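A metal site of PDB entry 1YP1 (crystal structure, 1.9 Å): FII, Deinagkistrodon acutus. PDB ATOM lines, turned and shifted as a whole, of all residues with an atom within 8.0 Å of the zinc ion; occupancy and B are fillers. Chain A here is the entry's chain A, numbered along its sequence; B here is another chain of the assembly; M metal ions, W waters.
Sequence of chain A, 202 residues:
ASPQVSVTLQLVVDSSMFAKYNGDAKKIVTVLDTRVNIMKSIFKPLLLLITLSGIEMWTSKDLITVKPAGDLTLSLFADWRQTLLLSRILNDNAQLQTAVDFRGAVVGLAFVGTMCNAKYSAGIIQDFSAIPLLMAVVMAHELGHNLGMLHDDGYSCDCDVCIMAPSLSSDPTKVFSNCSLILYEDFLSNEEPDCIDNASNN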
ATOM      1  N   GLY A 108     -21.152 -23.047  30.024  1.00  0.00           N
ATOM      2  CA  GLY A 108     -20.429 -21.844  29.643  1.00  0.00           C
ATOM      3  C   GLY A 108     -21.306 -20.595  29.735  1.00  0.00           C
ATOM      4  O   GLY A 108     -22.531 -20.693  29.605  1.00  0.00           O
ATOM      5  N   LEU A 109     -20.690 -19.439  29.965  1.00  0.00           N
ATOM      6  CA  LEU A 109     -21.438 -18.191  30.039  1.00  0.00           C
ATOM      7  C   LEU A 109     -20.538 -17.030  29.653  1.00  0.00           C
ATOM      8  O   LEU A 109     -19.309 -17.054  29.900  1.00  0.00           O
ATOM      9  CB  LEU A 109     -21.993 -18.007  31.464  1.00  0.00           C
ATOM     10  CG  LEU A 109     -23.268 -17.182  31.658  1.00  0.00           C
ATOM     11  CD1 LEU A 109     -24.474 -17.907  31.018  1.00  0.00           C
ATOM     12  CD2 LEU A 109     -23.524 -17.007  33.163  1.00  0.00           C
ATOM     13  N   ALA A 110     -21.140 -16.012  29.031  1.00  0.00           N
ATOM     14  CA  ALA A 110     -20.432 -14.819  28.581  1.00  0.00           C
ATOM     15  C   ALA A 110     -21.400 -13.664  28.416  1.00  0.00           C
ATOM     16  O   ALA A 110     -22.599 -13.883  28.280  1.00  0.00           O
ATOM     17  CB  ALA A 110     -19.750 -15.089  27.242  1.00  0.00           C
ATOM     18  N   VAL A 112     -22.924 -10.609  26.144  1.00  0.00           N
ATOM     19  CA  VAL A 112     -23.082 -10.422  24.707  1.00  0.00           C
ATOM     20  C   VAL A 112     -22.659  -9.054  24.150  1.00  0.00           C
ATOM     21  O   VAL A 112     -23.020  -8.019  24.714  1.00  0.00           O
ATOM     22  CB  VAL A 112     -24.544 -10.709  24.266  1.00  0.00           C
ATOM     23  CG1 VAL A 112     -24.624 -10.836  22.757  1.00  0.00           C
ATOM     24  CG2 VAL A 112     -25.032 -11.996  24.927  1.00  0.00           C
ATOM     25  N   VAL A 138     -17.324 -24.992  22.568  1.00  0.00           N
ATOM     26  CA  VAL A 138     -17.886 -24.346  23.755  1.00  0.00           C
ATOM     27  C   VAL A 138     -17.221 -22.988  23.999  1.00  0.00           C
ATOM     28  O   VAL A 138     -17.894 -21.979  24.281  1.00  0.00           O
ATOM     29  CB  VAL A 138     -17.708 -25.235  24.992  1.00  0.00           C
ATOM     30  CG1 VAL A 138     -18.273 -24.542  26.242  1.00  0.00           C
ATOM     31  CG2 VAL A 138     -18.388 -26.524  24.750  1.00  0.00           C
ATOM     32  N   HIS A 141     -18.307 -20.589  21.253  1.00  0.00           N
ATOM     33  CA  HIS A 141     -19.696 -20.128  21.393  1.00  0.00           C
ATOM     34  C   HIS A 141     -19.716 -18.915  22.335  1.00  0.00           C
ATOM     35  O   HIS A 141     -20.374 -17.902  22.066  1.00  0.00           O
ATOM     36  CB  HIS A 141     -20.544 -21.240  22.011  1.00  0.00           C
ATOM     37  CG  HIS A 141     -21.986 -20.883  22.219  1.00  0.00           C
ATOM     38  ND1 HIS A 141     -22.970 -21.245  21.314  1.00  0.00           N
ATOM     39  CD2 HIS A 141     -22.607 -20.226  23.221  1.00  0.00           C
ATOM     40  CE1 HIS A 141     -24.141 -20.831  21.764  1.00  0.00           C
ATOM     41  NE2 HIS A 141     -23.950 -20.217  22.913  1.00  0.00           N
ATOM     42  N   GLU A 142     -18.983 -19.014  23.441  1.00  0.00           N
ATOM     43  CA  GLU A 142     -18.920 -17.889  24.387  1.00  0.00           C
ATOM     44  C   GLU A 142     -18.219 -16.660  23.778  1.00  0.00           C
ATOM     45  O   GLU A 142     -18.652 -15.540  23.983  1.00  0.00           O
ATOM     46  CB  GLU A 142     -18.204 -18.297  25.672  1.00  0.00           C
ATOM     47  CG  GLU A 142     -18.892 -19.414  26.481  1.00  0.00           C
ATOM     48  CD  GLU A 142     -20.438 -19.289  26.550  1.00  0.00           C
ATOM     49  OE1 GLU A 142     -20.982 -18.177  26.628  1.00  0.00           O
ATOM     50  OE2 GLU A 142     -21.120 -20.339  26.556  1.00  0.00           O
ATOM     51  N   GLY A 144     -18.107 -16.029  20.710  1.00  0.00           N
ATOM     52  CA  GLY A 144     -19.003 -15.528  19.674  1.00  0.00           C
ATOM     53  C   GLY A 144     -20.035 -14.581  20.273  1.00  0.00           C
ATOM     54  O   GLY A 144     -20.367 -13.535  19.674  1.00  0.00           O
ATOM     55  N   HIS A 145     -20.542 -14.921  21.446  1.00  0.00           N
ATOM     56  CA  HIS A 145     -21.498 -14.027  22.114  1.00  0.00           C
ATOM     57  C   HIS A 145     -20.824 -12.699  22.414  1.00  0.00           C
ATOM     58  O   HIS A 145     -21.421 -11.639  22.246  1.00  0.00           O
ATOM     59  CB  HIS A 145     -21.992 -14.629  23.419  1.00  0.00           C
ATOM     60  CG  HIS A 145     -23.129 -15.580  23.232  1.00  0.00           C
ATOM     61  ND1 HIS A 145     -24.173 -15.340  22.361  1.00  0.00           N
ATOM     62  CD2 HIS A 145     -23.412 -16.759  23.840  1.00  0.00           C
ATOM     63  CE1 HIS A 145     -25.055 -16.323  22.442  1.00  0.00           C
ATOM     64  NE2 HIS A 145     -24.611 -17.197  23.337  1.00  0.00           N
ATOM     65  N   MET A 149     -22.722 -12.135  18.665  1.00  0.00           N
ATOM     66  CA  MET A 149     -23.557 -13.194  18.070  1.00  0.00           C
ATOM     67  C   MET A 149     -24.669 -13.675  18.965  1.00  0.00           C
ATOM     68  O   MET A 149     -24.456 -13.915  20.133  1.00  0.00           O
ATOM     69  CB  MET A 149     -22.716 -14.401  17.698  1.00  0.00           C
ATOM     70  CG  MET A 149     -21.679 -14.108  16.638  1.00  0.00           C
ATOM     71  SD  MET A 149     -20.723 -15.591  16.320  1.00  0.00           S
ATOM     72  CE  MET A 149     -19.582 -14.987  15.137  1.00  0.00           C
ATOM     73  N   LEU A 150     -25.865 -13.810  18.393  1.00  0.00           N
ATOM     74  CA  LEU A 150     -26.998 -14.345  19.155  1.00  0.00           C
ATOM     75  C   LEU A 150     -27.069 -15.807  18.755  1.00  0.00           C
ATOM     76  O   LEU A 150     -26.281 -16.265  17.925  1.00  0.00           O
ATOM     77  CB  LEU A 150     -28.290 -13.619  18.763  1.00  0.00           C
ATOM     78  CG  LEU A 150     -28.087 -12.097  18.850  1.00  0.00           C
ATOM     79  CD1 LEU A 150     -29.245 -11.391  18.206  1.00  0.00           C
ATOM     80  CD2 LEU A 150     -27.928 -11.694  20.305  1.00  0.00           C
ATOM     81  N   HIS A 151     -27.994 -16.548  19.362  1.00  0.00           N
ATOM     82  CA  HIS A 151     -28.151 -17.956  19.045  1.00  0.00           C
ATOM     83  C   HIS A 151     -28.726 -18.162  17.678  1.00  0.00           C
ATOM     84  O   HIS A 151     -29.438 -17.310  17.156  1.00  0.00           O
ATOM     85  CB  HIS A 151     -29.051 -18.633  20.065  1.00  0.00           C
ATOM     86  CG  HIS A 151     -28.416 -18.786  21.399  1.00  0.00           C
ATOM     87  ND1 HIS A 151     -29.123 -18.794  22.578  1.00  0.00           N
ATOM     88  CD2 HIS A 151     -27.119 -18.965  21.737  1.00  0.00           C
ATOM     89  CE1 HIS A 151     -28.281 -18.974  23.590  1.00  0.00           C
ATOM     90  NE2 HIS A 151     -27.059 -19.074  23.101  1.00  0.00           N
ATOM     91  N   ASP A 152     -28.382 -19.292  17.077  1.00  0.00           N
ATOM     92  CA  ASP A 152     -28.871 -19.631  15.759  1.00  0.00           C
ATOM     93  C   ASP A 152     -30.333 -20.048  15.858  1.00  0.00           C
ATOM     94  O   ASP A 152     -30.719 -20.733  16.794  1.00  0.00           O
ATOM     95  CB  ASP A 152     -28.144 -20.854  15.218  1.00  0.00           C
ATOM     96  CG  ASP A 152     -26.777 -20.541  14.714  1.00  0.00           C
ATOM     97  OD1 ASP A 152     -26.514 -19.380  14.327  1.00  0.00           O
ATOM     98  OD2 ASP A 152     -25.973 -21.488  14.654  1.00  0.00           O
ATOM     99  N   ILE A 163     -21.723 -23.379  15.497  1.00  0.00           N
ATOM    100  CA  ILE A 163     -21.232 -22.821  16.756  1.00  0.00           C
ATOM    101  C   ILE A 163     -22.283 -22.187  17.651  1.00  0.00           C
ATOM    102  O   ILE A 163     -22.352 -22.511  18.844  1.00  0.00           O
ATOM    103  CB  ILE A 163     -20.093 -21.735  16.525  1.00  0.00           C
ATOM    104  CG1 ILE A 163     -18.964 -22.334  15.682  1.00  0.00           C
ATOM    105  CG2 ILE A 163     -19.541 -21.239  17.893  1.00  0.00           C
ATOM    106  CD1 ILE A 163     -18.278 -23.547  16.315  1.00  0.00           C
ATOM    107  N   MET A 164     -23.107 -21.291  17.094  1.00  0.00           N
ATOM    108  CA  MET A 164     -24.073 -20.605  17.957  1.00  0.00           C
ATOM    109  C   MET A 164     -25.416 -21.261  18.240  1.00  0.00           C
ATOM    110  O   MET A 164     -26.364 -20.587  18.685  1.00  0.00           O
ATOM    111  CB  MET A 164     -24.273 -19.151  17.490  1.00  0.00           C
ATOM    112  CG  MET A 164     -22.956 -18.372  17.358  1.00  0.00           C
ATOM    113  SD  MET A 164     -22.027 -18.358  18.946  1.00  0.00           S
ATOM    114  CE  MET A 164     -23.176 -17.590  20.075  1.00  0.00           C
ATOM    115  N   ALA A 165     -25.493 -22.579  18.043  1.00  0.00           N
ATOM    116  CA  ALA A 165     -26.706 -23.313  18.382  1.00  0.00           C
ATOM    117  C   ALA A 165     -26.835 -23.141  19.892  1.00  0.00           C
ATOM    118  O   ALA A 165     -25.837 -23.201  20.621  1.00  0.00           O
ATOM    119  CB  ALA A 165     -26.538 -24.772  18.042  1.00  0.00           C
ATOM    120  N   PRO A 166     -28.064 -22.924  20.401  1.00  0.00           N
ATOM    121  CA  PRO A 166     -28.362 -22.718  21.830  1.00  0.00           C
ATOM    122  C   PRO A 166     -27.805 -23.819  22.748  1.00  0.00           C
ATOM    123  O   PRO A 166     -27.383 -23.568  23.879  1.00  0.00           O
ATOM    124  CB  PRO A 166     -29.886 -22.675  21.855  1.00  0.00           C
ATOM    125  CG  PRO A 166     -30.231 -22.148  20.516  1.00  0.00           C
ATOM    126  CD  PRO A 166     -29.303 -22.900  19.604  1.00  0.00           C
ATOM    127  N   SER A 167     -27.812 -25.043  22.244  1.00  0.00           N
ATOM    128  CA  SER A 167     -27.289 -26.176  23.004  1.00  0.00           C
ATOM    129  C   SER A 167     -26.171 -26.779  22.191  1.00  0.00           C
ATOM    130  O   SER A 167     -26.250 -26.847  20.966  1.00  0.00           O
ATOM    131  CB  SER A 167     -28.371 -27.228  23.245  1.00  0.00           C
ATOM    132  OG  SER A 167     -29.310 -26.796  24.238  1.00  0.00           O
ATOM    133  N   ASN B   2     -25.808 -26.751  27.751  1.00  0.00           N
ATOM    134  CA  ASN B   2     -26.195 -25.358  27.535  1.00  0.00           C
ATOM    135  C   ASN B   2     -25.032 -24.346  27.563  1.00  0.00           C
ATOM    136  O   ASN B   2     -24.336 -24.189  28.562  1.00  0.00           O
ATOM    137  CB  ASN B   2     -27.258 -24.968  28.567  1.00  0.00           C
ATOM    138  CG  ASN B   2     -28.207 -23.928  28.041  1.00  0.00           C
ATOM    139  OD1 ASN B   2     -28.997 -23.369  28.801  1.00  0.00           O
ATOM    140  ND2 ASN B   2     -28.166 -23.673  26.741  1.00  0.00           N
ATOM    141  N   LEU B   3     -24.799 -23.640  26.482  1.00  0.00           N
ATOM    142  CA  LEU B   3     -23.642 -22.747  26.557  1.00  0.00           C
ATOM    143  C   LEU B   3     -23.966 -21.303  26.767  1.00  0.00           C
ATOM    144  O   LEU B   3     -23.888 -20.527  25.786  1.00  0.00           O
ATOM    145  CB  LEU B   3     -22.754 -22.906  25.346  1.00  0.00           C
ATOM    146  CG  LEU B   3     -22.963 -24.257  24.682  1.00  0.00           C
ATOM    147  CD1 LEU B   3     -23.818 -24.007  23.483  1.00  0.00           C
ATOM    148  CD2 LEU B   3     -21.627 -24.904  24.324  1.00  0.00           C
ATOM    149  OXT LEU B   3     -24.284 -20.960  27.917  1.00  0.00           O
HETATM  150 ZN    ZN M   1     -25.304 -19.126  24.137  1.00  0.00          ZN
HETATM  151  O   HOH W   1     -26.375 -20.870  25.170  1.00  0.00           O
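The backbone carbonyl oxygen of Ile 163 sits at hydrogen-bond distance from a ring nitrogen (ND1) of His 141 (2.8 Å).
O of Met 149 sits at hydrogen-bond distance from ND1 of His 145 (2.7 Å).
OXT of Leu 3 of chain B lies close to O of Gly 108 (2.4 Å).
Four residues have an atom within 4 Å of the zinc ion: His 141, His 145, His 151 and Leu 3 of chain B.
The nearest printed residue that does not touch the zinc ion is Met 164 (4.8 Å).
The zinc ion is bound by a ring nitrogen (NE2) of His 151 (2.0 Å), a ring nitrogen (NE2) of His 141 (2.1 Å), a ring nitrogen (NE2) of His 145 (2.2 Å), water W1 (2.3 Å) and the chain-end carboxylate of Leu 3 of chain B (2.6 Å).
Water W1 bridges the backbone carbonyl oxygen of Pro 166 (3.2 Å) and the backbone NH of Leu 3 of chain B (3.4 Å).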
